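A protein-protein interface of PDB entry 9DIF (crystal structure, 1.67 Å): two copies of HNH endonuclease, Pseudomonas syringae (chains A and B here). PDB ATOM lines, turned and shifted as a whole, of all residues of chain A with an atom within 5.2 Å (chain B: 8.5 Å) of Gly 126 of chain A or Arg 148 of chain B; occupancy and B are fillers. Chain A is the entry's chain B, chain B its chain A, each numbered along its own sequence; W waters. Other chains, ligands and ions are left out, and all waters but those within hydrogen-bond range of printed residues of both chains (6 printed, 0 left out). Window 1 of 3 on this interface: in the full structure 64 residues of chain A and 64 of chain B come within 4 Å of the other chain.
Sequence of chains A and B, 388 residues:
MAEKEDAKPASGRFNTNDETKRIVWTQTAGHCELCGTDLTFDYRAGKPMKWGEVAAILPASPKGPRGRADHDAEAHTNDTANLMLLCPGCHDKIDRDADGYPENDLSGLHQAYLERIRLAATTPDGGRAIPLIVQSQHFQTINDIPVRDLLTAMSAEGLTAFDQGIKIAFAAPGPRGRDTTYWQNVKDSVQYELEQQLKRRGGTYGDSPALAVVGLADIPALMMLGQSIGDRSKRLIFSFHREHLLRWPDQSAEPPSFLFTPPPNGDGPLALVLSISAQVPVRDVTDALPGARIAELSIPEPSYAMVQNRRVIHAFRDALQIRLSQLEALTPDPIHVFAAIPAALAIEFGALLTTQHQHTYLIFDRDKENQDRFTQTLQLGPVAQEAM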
ATOM      1  N   LEU A 119      18.350  -9.409   2.883  1.00  0.00           N
ATOM      2  CA  LEU A 119      19.714  -9.685   3.283  1.00  0.00           C
ATOM      3  C   LEU A 119      19.842 -11.128   3.675  1.00  0.00           C
ATOM      4  O   LEU A 119      20.834 -11.777   3.340  1.00  0.00           O
ATOM      5  CB  LEU A 119      20.117  -8.772   4.431  1.00  0.00           C
ATOM      6  CG  LEU A 119      21.581  -8.782   4.828  1.00  0.00           C
ATOM      7  CD1 LEU A 119      22.537  -8.301   3.774  1.00  0.00           C
ATOM      8  CD2 LEU A 119      21.710  -7.907   6.032  1.00  0.00           C
ATOM      9  N   THR A 122      19.453 -13.496   0.525  1.00  0.00           N
ATOM     10  CA  THR A 122      20.567 -13.488  -0.392  1.00  0.00           C
ATOM     11  C   THR A 122      21.827 -14.054   0.244  1.00  0.00           C
ATOM     12  O   THR A 122      22.828 -14.208  -0.448  1.00  0.00           O
ATOM     13  CB  THR A 122      20.836 -12.076  -0.906  1.00  0.00           C
ATOM     14  OG1 THR A 122      21.080 -11.212   0.208  1.00  0.00           O
ATOM     15  CG2 THR A 122      19.682 -11.535  -1.700  1.00  0.00           C
ATOM     16  N   THR A 123      21.758 -14.470   1.511  1.00  0.00           N
ATOM     17  CA  THR A 123      22.936 -14.969   2.211  1.00  0.00           C
ATOM     18  C   THR A 123      23.681 -16.100   1.509  1.00  0.00           C
ATOM     19  O   THR A 123      24.917 -16.152   1.607  1.00  0.00           O
ATOM     20  CB  THR A 123      22.523 -15.400   3.608  1.00  0.00           C
ATOM     21  OG1 THR A 123      22.062 -14.253   4.331  1.00  0.00           O
ATOM     22  CG2 THR A 123      23.725 -15.948   4.356  1.00  0.00           C
ATOM     23  N   PRO A 124      23.013 -17.007   0.764  1.00  0.00           N
ATOM     24  CA  PRO A 124      23.770 -18.034   0.027  1.00  0.00           C
ATOM     25  C   PRO A 124      24.763 -17.470  -0.975  1.00  0.00           C
ATOM     26  O   PRO A 124      25.723 -18.180  -1.306  1.00  0.00           O
ATOM     27  CB  PRO A 124      22.666 -18.861  -0.647  1.00  0.00           C
ATOM     28  CG  PRO A 124      21.411 -18.645   0.330  1.00  0.00           C
ATOM     29  CD  PRO A 124      21.564 -17.295   0.835  1.00  0.00           C
ATOM     30  N   ASP A 125      24.560 -16.270  -1.528  1.00  0.00           N
ATOM     31  CA  ASP A 125      25.614 -15.823  -2.444  1.00  0.00           C
ATOM     32  C   ASP A 125      26.833 -15.293  -1.672  1.00  0.00           C
ATOM     33  O   ASP A 125      27.917 -15.095  -2.256  1.00  0.00           O
ATOM     34  CB  ASP A 125      25.063 -14.803  -3.481  1.00  0.00           C
ATOM     35  CG  ASP A 125      24.983 -13.331  -2.957  1.00  0.00           C
ATOM     36  OD1 ASP A 125      25.847 -12.796  -2.179  1.00  0.00           O
ATOM     37  OD2 ASP A 125      24.025 -12.655  -3.398  1.00  0.00           O
ATOM     38  N   GLY A 126      26.677 -15.068  -0.360  1.00  0.00           N
ATOM     39  CA  GLY A 126      27.841 -14.823   0.476  1.00  0.00           C
ATOM     40  C   GLY A 126      28.806 -15.997   0.571  1.00  0.00           C
ATOM     41  O   GLY A 126      29.876 -15.858   1.186  1.00  0.00           O
ATOM     42  N   GLY A 127      28.463 -17.153  -0.022  1.00  0.00           N
ATOM     43  CA  GLY A 127      29.331 -18.326  -0.037  1.00  0.00           C
ATOM     44  C   GLY A 127      30.312 -18.433  -1.209  1.00  0.00           C
ATOM     45  O   GLY A 127      31.076 -19.402  -1.287  1.00  0.00           O
ATOM     46  N   ARG A 128      30.280 -17.480  -2.145  1.00  0.00           N
ATOM     47  CA  ARG A 128      31.130 -17.542  -3.328  1.00  0.00           C
ATOM     48  C   ARG A 128      32.561 -17.724  -2.849  1.00  0.00           C
ATOM     49  O   ARG A 128      32.971 -17.028  -1.916  1.00  0.00           O
ATOM     50  CB  ARG A 128      31.019 -16.264  -4.160  1.00  0.00           C
ATOM     51  CG  ARG A 128      29.767 -16.214  -5.015  1.00  0.00           C
ATOM     52  CD  ARG A 128      29.715 -14.970  -5.943  1.00  0.00           C
ATOM     53  NE  ARG A 128      30.564 -15.049  -7.122  1.00  0.00           N
ATOM     54  CZ  ARG A 128      31.750 -14.444  -7.268  1.00  0.00           C
ATOM     55  NH1 ARG A 128      32.309 -13.779  -6.268  1.00  0.00           N
ATOM     56  NH2 ARG A 128      32.392 -14.557  -8.426  1.00  0.00           N
ATOM     57  N   THR A 204      25.911  -9.965  -4.246  1.00  0.00           N
ATOM     58  CA  THR A 204      24.984  -8.859  -4.098  1.00  0.00           C
ATOM     59  C   THR A 204      25.724  -7.533  -3.954  1.00  0.00           C
ATOM     60  O   THR A 204      25.229  -6.496  -4.410  1.00  0.00           O
ATOM     61  CB  THR A 204      24.057  -9.121  -2.911  1.00  0.00           C
ATOM     62  OG1 THR A 204      23.244 -10.264  -3.206  1.00  0.00           O
ATOM     63  CG2 THR A 204      23.177  -7.905  -2.703  1.00  0.00           C
ATOM     64  N   TYR A 205      26.919  -7.550  -3.363  1.00  0.00           N
ATOM     65  CA  TYR A 205      27.607  -6.319  -2.992  1.00  0.00           C
ATOM     66  C   TYR A 205      28.948  -6.116  -3.664  1.00  0.00           C
ATOM     67  O   TYR A 205      29.618  -5.109  -3.400  1.00  0.00           O
ATOM     68  CB  TYR A 205      27.774  -6.290  -1.469  1.00  0.00           C
ATOM     69  CG  TYR A 205      26.434  -6.391  -0.773  1.00  0.00           C
ATOM     70  CD1 TYR A 205      25.555  -5.308  -0.750  1.00  0.00           C
ATOM     71  CD2 TYR A 205      26.039  -7.573  -0.149  1.00  0.00           C
ATOM     72  CE1 TYR A 205      24.301  -5.407  -0.104  1.00  0.00           C
ATOM     73  CE2 TYR A 205      24.838  -7.684   0.465  1.00  0.00           C
ATOM     74  CZ  TYR A 205      23.940  -6.602   0.472  1.00  0.00           C
ATOM     75  OH  TYR A 205      22.705  -6.698   1.094  1.00  0.00           O
ATOM     76  N   ASP A 207      31.587  -8.155  -3.226  1.00  0.00           N
ATOM     77  CA  ASP A 207      32.636  -8.677  -2.361  1.00  0.00           C
ATOM     78  C   ASP A 207      33.572  -9.613  -3.116  1.00  0.00           C
ATOM     79  O   ASP A 207      33.165 -10.382  -4.000  1.00  0.00           O
ATOM     80  CB  ASP A 207      32.036  -9.407  -1.143  1.00  0.00           C
ATOM     81  CG  ASP A 207      31.446  -8.450  -0.069  1.00  0.00           C
ATOM     82  OD1 ASP A 207      31.875  -7.270  -0.024  1.00  0.00           O
ATOM     83  OD2 ASP A 207      30.539  -8.871   0.698  1.00  0.00           O
ATOM     84  N   LYS A 234      37.862 -13.162   4.556  1.00  0.00           N
ATOM     85  CA  LYS A 234      36.989 -14.324   4.698  1.00  0.00           C
ATOM     86  C   LYS A 234      37.707 -15.555   4.145  1.00  0.00           C
ATOM     87  O   LYS A 234      37.942 -15.681   2.935  1.00  0.00           O
ATOM     88  CB  LYS A 234      35.639 -14.107   4.021  1.00  0.00           C
ATOM     89  CG  LYS A 234      34.717 -15.333   4.240  1.00  0.00           C
ATOM     90  CD  LYS A 234      33.245 -14.980   3.922  1.00  0.00           C
ATOM     91  CE  LYS A 234      32.373 -16.193   4.019  1.00  0.00           C
ATOM     92  NZ  LYS A 234      30.904 -15.858   3.888  1.00  0.00           N
ATOM     93  N   HIS B  31      13.453 -16.778  -2.848  1.00  0.00           N
ATOM     94  CA  HIS B  31      14.822 -16.861  -3.323  1.00  0.00           C
ATOM     95  C   HIS B  31      15.337 -18.296  -3.339  1.00  0.00           C
ATOM     96  O   HIS B  31      14.924 -19.132  -2.526  1.00  0.00           O
ATOM     97  CB  HIS B  31      15.797 -16.025  -2.457  1.00  0.00           C
ATOM     98  CG  HIS B  31      15.690 -14.524  -2.649  1.00  0.00           C
ATOM     99  ND1 HIS B  31      14.545 -13.822  -2.381  1.00  0.00           N
ATOM    100  CD2 HIS B  31      16.601 -13.616  -3.085  1.00  0.00           C
ATOM    101  CE1 HIS B  31      14.752 -12.529  -2.605  1.00  0.00           C
ATOM    102  NE2 HIS B  31      15.985 -12.383  -3.039  1.00  0.00           N
ATOM    103  N   LEU B  34      19.913 -22.369  -2.399  1.00  0.00           N
ATOM    104  CA  LEU B  34      21.281 -22.752  -2.634  1.00  0.00           C
ATOM    105  C   LEU B  34      22.138 -21.633  -3.238  1.00  0.00           C
ATOM    106  O   LEU B  34      23.354 -21.651  -3.030  1.00  0.00           O
ATOM    107  CB  LEU B  34      21.312 -24.007  -3.522  1.00  0.00           C
ATOM    108  CG  LEU B  34      20.892 -25.293  -2.827  1.00  0.00           C
ATOM    109  CD1 LEU B  34      20.844 -26.443  -3.792  1.00  0.00           C
ATOM    110  CD2 LEU B  34      21.916 -25.697  -1.698  1.00  0.00           C
ATOM    111  N   CYS B  35      21.571 -20.614  -3.916  1.00  0.00           N
ATOM    112  CA  CYS B  35      22.429 -19.555  -4.478  1.00  0.00           C
ATOM    113  C   CYS B  35      21.914 -18.147  -4.192  1.00  0.00           C
ATOM    114  O   CYS B  35      22.637 -17.179  -4.460  1.00  0.00           O
ATOM    115  CB  CYS B  35      22.651 -19.760  -6.002  1.00  0.00           C
ATOM    116  SG  CYS B  35      21.151 -19.342  -6.983  1.00  0.00           S
ATOM    117  N   GLY B  36      20.718 -17.986  -3.641  1.00  0.00           N
ATOM    118  CA  GLY B  36      20.310 -16.688  -3.197  1.00  0.00           C
ATOM    119  C   GLY B  36      19.702 -15.836  -4.269  1.00  0.00           C
ATOM    120  O   GLY B  36      19.317 -14.717  -3.968  1.00  0.00           O
ATOM    121  N   ARG B 116      17.569 -18.550   9.094  1.00  0.00           N
ATOM    122  CA  ARG B 116      18.041 -17.178   8.942  1.00  0.00           C
ATOM    123  C   ARG B 116      16.903 -16.237   8.568  1.00  0.00           C
ATOM    124  O   ARG B 116      16.867 -15.079   9.015  1.00  0.00           O
ATOM    125  CB  ARG B 116      19.127 -17.141   7.869  1.00  0.00           C
ATOM    126  CG  ARG B 116      20.444 -17.723   8.317  1.00  0.00           C
ATOM    127  CD  ARG B 116      21.595 -17.410   7.334  1.00  0.00           C
ATOM    128  NE  ARG B 116      21.410 -18.020   6.019  1.00  0.00           N
ATOM    129  CZ  ARG B 116      21.968 -19.163   5.640  1.00  0.00           C
ATOM    130  NH1 ARG B 116      22.806 -19.819   6.440  1.00  0.00           N
ATOM    131  NH2 ARG B 116      21.662 -19.662   4.441  1.00  0.00           N
ATOM    132  N   ILE B 133      33.375   0.908   6.284  1.00  0.00           N
ATOM    133  CA  ILE B 133      34.544   0.014   6.323  1.00  0.00           C
ATOM    134  C   ILE B 133      35.804   0.817   5.990  1.00  0.00           C
ATOM    135  O   ILE B 133      35.906   1.371   4.898  1.00  0.00           O
ATOM    136  CB  ILE B 133      34.416  -1.160   5.330  1.00  0.00           C
ATOM    137  CG1 ILE B 133      33.257  -2.037   5.781  1.00  0.00           C
ATOM    138  CG2 ILE B 133      35.711  -2.006   5.321  1.00  0.00           C
ATOM    139  CD1 ILE B 133      32.902  -3.069   4.789  1.00  0.00           C
ATOM    140  N   ILE B 145      37.666  -6.674   4.383  1.00  0.00           N
ATOM    141  CA  ILE B 145      36.449  -6.856   5.177  1.00  0.00           C
ATOM    142  C   ILE B 145      35.265  -7.003   4.227  1.00  0.00           C
ATOM    143  O   ILE B 145      34.994  -6.081   3.445  1.00  0.00           O
ATOM    144  CB  ILE B 145      36.234  -5.675   6.125  1.00  0.00           C
ATOM    145  CG1 ILE B 145      37.389  -5.615   7.102  1.00  0.00           C
ATOM    146  CG2 ILE B 145      34.938  -5.828   6.880  1.00  0.00           C
ATOM    147  CD1 ILE B 145      37.433  -4.277   7.854  1.00  0.00           C
ATOM    148  N   PRO B 146      34.554  -8.123   4.241  1.00  0.00           N
ATOM    149  CA  PRO B 146      33.383  -8.234   3.362  1.00  0.00           C
ATOM    150  C   PRO B 146      32.249  -7.274   3.749  1.00  0.00           C
ATOM    151  O   PRO B 146      31.886  -7.131   4.919  1.00  0.00           O
ATOM    152  CB  PRO B 146      32.971  -9.708   3.512  1.00  0.00           C
ATOM    153  CG  PRO B 146      34.087 -10.374   4.166  1.00  0.00           C
ATOM    154  CD  PRO B 146      34.762  -9.356   5.020  1.00  0.00           C
ATOM    155  N   VAL B 147      31.653  -6.613   2.745  1.00  0.00           N
ATOM    156  CA  VAL B 147      30.500  -5.745   2.996  1.00  0.00           C
ATOM    157  C   VAL B 147      29.321  -6.525   3.557  1.00  0.00           C
ATOM    158  O   VAL B 147      28.661  -6.085   4.500  1.00  0.00           O
ATOM    159  CB  VAL B 147      30.101  -5.004   1.709  1.00  0.00           C
ATOM    160  CG1 VAL B 147      28.877  -4.217   1.890  1.00  0.00           C
ATOM    161  CG2 VAL B 147      31.235  -4.079   1.254  1.00  0.00           C
ATOM    162  N   ARG B 148      29.047  -7.710   3.001  1.00  0.00           N
ATOM    163  CA  ARG B 148      27.887  -8.479   3.431  1.00  0.00           C
ATOM    164  C   ARG B 148      27.975  -8.751   4.933  1.00  0.00           C
ATOM    165  O   ARG B 148      26.971  -8.707   5.664  1.00  0.00           O
ATOM    166  CB  ARG B 148      27.794  -9.792   2.626  1.00  0.00           C
ATOM    167  CG  ARG B 148      26.618 -10.727   3.188  1.00  0.00           C
ATOM    168  CD  ARG B 148      26.343 -12.007   2.355  1.00  0.00           C
ATOM    169  NE  ARG B 148      25.744 -11.702   1.064  1.00  0.00           N
ATOM    170  CZ  ARG B 148      24.452 -11.480   0.899  1.00  0.00           C
ATOM    171  NH1 ARG B 148      23.619 -11.507   1.930  1.00  0.00           N
ATOM    172  NH2 ARG B 148      23.985 -11.204  -0.322  1.00  0.00           N
ATOM    173  N   ASP B 149      29.172  -9.055   5.405  1.00  0.00           N
ATOM    174  CA  ASP B 149      29.276  -9.402   6.816  1.00  0.00           C
ATOM    175  C   ASP B 149      29.011  -8.235   7.762  1.00  0.00           C
ATOM    176  O   ASP B 149      28.478  -8.465   8.857  1.00  0.00           O
ATOM    177  CB  ASP B 149      30.637 -10.005   7.139  1.00  0.00           C
ATOM    178  CG  ASP B 149      30.814 -11.388   6.508  1.00  0.00           C
ATOM    179  OD1 ASP B 149      31.042 -11.486   5.279  1.00  0.00           O
ATOM    180  OD2 ASP B 149      30.698 -12.392   7.251  1.00  0.00           O
ATOM    181  N   LEU B 150      29.376  -7.000   7.402  1.00  0.00           N
ATOM    182  CA  LEU B 150      29.024  -5.845   8.222  1.00  0.00           C
ATOM    183  C   LEU B 150      27.529  -5.606   8.200  1.00  0.00           C
ATOM    184  O   LEU B 150      26.906  -5.411   9.238  1.00  0.00           O
ATOM    185  CB  LEU B 150      29.746  -4.588   7.736  1.00  0.00           C
ATOM    186  CG  LEU B 150      29.276  -3.277   8.380  1.00  0.00           C
ATOM    187  CD1 LEU B 150      29.482  -3.301   9.889  1.00  0.00           C
ATOM    188  CD2 LEU B 150      30.048  -2.071   7.829  1.00  0.00           C
ATOM    189  N   LEU B 151      26.932  -5.618   6.988  1.00  0.00           N
ATOM    190  CA  LEU B 151      25.477  -5.421   6.824  1.00  0.00           C
ATOM    191  C   LEU B 151      24.705  -6.479   7.606  1.00  0.00           C
ATOM    192  O   LEU B 151      23.642  -6.190   8.190  1.00  0.00           O
ATOM    193  CB  LEU B 151      25.099  -5.470   5.347  1.00  0.00           C
ATOM    194  CG  LEU B 151      25.643  -4.292   4.548  1.00  0.00           C
ATOM    195  CD1 LEU B 151      25.327  -4.511   3.066  1.00  0.00           C
ATOM    196  CD2 LEU B 151      25.142  -2.991   4.981  1.00  0.00           C
ATOM    197  N   THR B 152      25.282  -7.671   7.718  1.00  0.00           N
ATOM    198  CA  THR B 152      24.605  -8.761   8.417  1.00  0.00           C
ATOM    199  C   THR B 152      24.698  -8.578   9.920  1.00  0.00           C
ATOM    200  O   THR B 152      23.727  -8.832  10.655  1.00  0.00           O
ATOM    201  CB  THR B 152      25.204 -10.112   7.993  1.00  0.00           C
ATOM    202  OG1 THR B 152      25.102 -10.287   6.564  1.00  0.00           O
ATOM    203  CG2 THR B 152      24.482 -11.305   8.608  1.00  0.00           C
ATOM    204  N   ALA B 153      25.852  -8.157  10.415  1.00  0.00           N
ATOM    205  CA  ALA B 153      25.981  -7.802  11.818  1.00  0.00           C
ATOM    206  C   ALA B 153      25.076  -6.636  12.176  1.00  0.00           C
ATOM    207  O   ALA B 153      24.525  -6.545  13.288  1.00  0.00           O
ATOM    208  CB  ALA B 153      27.456  -7.509  12.093  1.00  0.00           C
ATOM    209  N   MET B 154      24.979  -5.650  11.290  1.00  0.00           N
ATOM    210  CA  MET B 154      24.057  -4.563  11.515  1.00  0.00           C
ATOM    211  C   MET B 154      22.647  -5.099  11.654  1.00  0.00           C
ATOM    212  O   MET B 154      21.909  -4.735  12.577  1.00  0.00           O
ATOM    213  CB  MET B 154      24.170  -3.583  10.351  1.00  0.00           C
ATOM    214  CG  MET B 154      25.479  -2.785  10.333  1.00  0.00           C
ATOM    215  SD  MET B 154      25.600  -1.689   8.900  1.00  0.00           S
ATOM    216  CE  MET B 154      24.049  -0.764   8.922  1.00  0.00           C
ATOM    217  N   SER B 155      22.241  -5.942  10.693  1.00  0.00           N
ATOM    218  CA  SER B 155      20.876  -6.444  10.656  1.00  0.00           C
ATOM    219  C   SER B 155      20.548  -7.310  11.882  1.00  0.00           C
ATOM    220  O   SER B 155      19.390  -7.342  12.349  1.00  0.00           O
ATOM    221  CB  SER B 155      20.666  -7.241   9.377  1.00  0.00           C
ATOM    222  OG  SER B 155      19.334  -7.674   9.408  1.00  0.00           O
ATOM    223  N   GLN B 164      24.813   0.147   0.441  1.00  0.00           N
ATOM    224  CA  GLN B 164      25.807  -0.694   1.084  1.00  0.00           C
ATOM    225  C   GLN B 164      26.898   0.116   1.785  1.00  0.00           C
ATOM    226  O   GLN B 164      27.793  -0.475   2.402  1.00  0.00           O
ATOM    227  CB  GLN B 164      26.421  -1.628   0.050  1.00  0.00           C
ATOM    228  CG  GLN B 164      27.302  -1.024  -1.051  1.00  0.00           C
ATOM    229  CD  GLN B 164      28.010  -2.118  -1.858  1.00  0.00           C
ATOM    230  OE1 GLN B 164      29.190  -2.415  -1.628  1.00  0.00           O
ATOM    231  NE2 GLN B 164      27.269  -2.774  -2.738  1.00  0.00           N
ATOM    232  N   LYS B 167      33.326   2.278   1.683  1.00  0.00           N
ATOM    233  CA  LYS B 167      34.428   1.352   1.937  1.00  0.00           C
ATOM    234  C   LYS B 167      35.707   2.024   1.476  1.00  0.00           C
ATOM    235  O   LYS B 167      35.873   2.258   0.282  1.00  0.00           O
ATOM    236  CB  LYS B 167      34.273  -0.003   1.238  1.00  0.00           C
ATOM    237  CG  LYS B 167      35.433  -1.014   1.533  1.00  0.00           C
ATOM    238  CD  LYS B 167      34.991  -2.437   1.320  1.00  0.00           C
ATOM    239  CE  LYS B 167      36.138  -3.423   1.390  1.00  0.00           C
ATOM    240  NZ  LYS B 167      35.596  -4.860   1.127  1.00  0.00           N
ATOM    241  N   LEU B 245      34.674 -13.286  12.492  1.00  0.00           N
ATOM    242  CA  LEU B 245      34.569 -12.226  11.459  1.00  0.00           C
ATOM    243  C   LEU B 245      33.842 -11.031  12.038  1.00  0.00           C
ATOM    244  O   LEU B 245      34.327 -10.489  13.055  1.00  0.00           O
ATOM    245  CB  LEU B 245      33.958 -12.829  10.194  1.00  0.00           C
ATOM    246  CG  LEU B 245      34.796 -13.753   9.340  1.00  0.00           C
ATOM    247  CD1 LEU B 245      34.083 -13.955   8.022  1.00  0.00           C
ATOM    248  CD2 LEU B 245      36.186 -13.238   9.129  1.00  0.00           C
ATOM    249  N   LEU B 246      32.633 -10.635  11.548  1.00  0.00           N
ATOM    250  CA  LEU B 246      31.911  -9.448  12.026  1.00  0.00           C
ATOM    251  C   LEU B 246      30.867  -9.766  13.082  1.00  0.00           C
ATOM    252  O   LEU B 246      30.320  -8.857  13.735  1.00  0.00           O
ATOM    253  CB  LEU B 246      31.246  -8.722  10.860  1.00  0.00           C
ATOM    254  CG  LEU B 246      32.054  -7.506  10.377  1.00  0.00           C
ATOM    255  CD1 LEU B 246      31.902  -6.401  11.427  1.00  0.00           C
ATOM    256  CD2 LEU B 246      33.488  -7.804  10.026  1.00  0.00           C
HETATM  257  O   HOH W   1      25.790 -20.468  -3.799  1.00  0.00           O
HETATM  258  O   HOH W   2      33.686  -5.331  -0.979  1.00  0.00           O
HETATM  259  O   HOH W   3      28.104 -11.418  -0.894  1.00  0.00           O
HETATM  260  O   HOH W   4      30.412 -14.982   6.592  1.00  0.00           O
HETATM  261  O   HOH W   5      30.129 -12.936   3.303  1.00  0.00           O
HETATM  262  O   HOH W   6      23.877 -12.153   4.478  1.00  0.00           O
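No position is printed for both chains.
CD2 of Leu 119 of chain A touches O of Leu 151 of chain B, at 3.4 Å.
Leu 119 of chain A touches Ser 155 of chain B.
CG2 of Thr 122 of chain A touches O of Gly 36 of chain B (3.9 Å).
Arg 148 of chain B touches Thr 123 of chain A (NH1 to N, 3.5 Å).
O of Leu 34 of chain B touches CB of Pro 124 of chain A, 3.7 Å away.
Pro 124 of chain A touches Cys 35 of chain B.
Gly 36 of chain B touches Pro 124 of chain A (N to CB, 3.7 Å).
Cys 35 of chain B touches Asp 125 of chain A (O to CB, 3.5 Å).
CD of Arg 148 of chain B touches CA of Gly 126 of chain A (3.7 Å).
OD1 of Asp 207 of chain A touches C of Pro 146 of chain B, 3.8 Å away.
The guanidinium group (NH1) of Arg 148 of chain B lies within hydrogen-bond range of the backbone carbonyl oxygen (O) of Leu 119 of chain A, at 3.1 Å.
The guanidinium group (NH2) of Arg 148 of chain B lies within hydrogen-bond range of the side-chain hydroxyl (OG1) of Thr 204 of chain A (3.1 Å).
The guanidinium group (NH2) of Arg 148 of chain B lies within salt-bridge range of the side-chain carboxylate (OD1) of Asp 125 of chain A, at 3.1 Å.
OD1 of Asp 207 of chain A is in hydrogen-bond range of N of Val 147 of chain B (2.9 Å).
The side-chain carboxylate (OD2) of Asp 207 of chain A is in hydrogen-bond range of the backbone NH (N) of Arg 148 of chain B, 3.0 Å away.
NH2 of Arg 148 of chain B is in hydrogen-bond range of OG1 of Thr 122 of chain A (3.0 Å).
The side-chain amide oxygen (OE1) of Gln 164 of chain B sits close to the backbone carbonyl oxygen (O) of Tyr 205 of chain A.
The side-chain carboxylate (OD2) of Asp 125 of chain A sits at hydrogen-bond distance from the side-chain hydroxyl (OG1) of Thr 204 of chain A (2.5 Å).
O of Leu 119 of chain A lies within hydrogen-bond range of OG1 of Thr 123 of chain A.
O of Leu 119 of chain A is in hydrogen-bond range of OG1 of Thr 122 of chain A, at 3.2 Å.
The backbone carbonyl oxygen of Arg 148 of chain B lies within hydrogen-bond range of the side-chain hydroxyl of Thr 152 of chain B (2.6 Å).
O of Gly 126 of chain A sits at hydrogen-bond distance from NZ of Lys 234 of chain A (2.9 Å).
Of chain B, only Cys 35 and Arg 148 come within 4 Å of Asp 125 of chain A.
Printed residues of chain B within 4 Å of Gly 126 of chain A: Arg 148 (3.7 Å).
Of the printed residues of chain A, Leu 34 of chain B touches Pro 124.
Of the printed residues of chain A, Gly 36 of chain B touches Thr 122 (3.9 Å) and Pro 124 (3.7 Å).
Ile 145 of chain B touches none of the printed residues of chain A.
Of the printed residues of chain A, Val 147 of chain B touches Asp 207.
Of the printed residues of chain A, Arg 148 of chain B touches Leu 119 (3.1 Å), Thr 122 (3.0 Å), Thr 123 (3.5 Å), Asp 125 (3.1 Å), Gly 126 (3.7 Å), Thr 204 (3.1 Å), Tyr 205 (3.7 Å) and Asp 207 (3.0 Å).
The nearest printed residue of chain B that does not touch Gly 126 of chain A is Asp 149 of chain B (6.1 Å).
Water W5 bridges OD1 of Asp 149 of chain B (2.6 Å) and NZ of Lys 234 of chain A (3.1 Å).
Water W6 lies within hydrogen-bond range of the guanidinium group (NH1) of Arg 148 of chain B, the side-chain hydroxyl (OG1) of Thr 123 of chain A, the side-chain hydroxyl (OG1) of Thr 152 of chain B and the backbone carbonyl oxygen (O) of Leu 119 of chain A.
Water W4 lies within hydrogen-bond range of the side-chain carboxylate (OD2) of Asp 149 of chain B (2.7 Å) and the side-chain amino group (NZ) of Lys 234 of chain A (2.9 Å).
Water W1 lies within hydrogen-bond range of O of Leu 34 of chain B (2.8 Å) and O of Pro 124 of chain A (3.4 Å).
Water W2 bridges the side-chain carboxylate of Asp 207 of chain A (2.8 Å) and the side-chain amino group of Lys 167 of chain B (2.9 Å).
Water W3 lies within hydrogen-bond range of the side-chain carboxylate (OD1) of Asp 125 of chain A (2.9 Å) and the guanidinium group (NE) of Arg 148 of chain B (3.1 Å).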
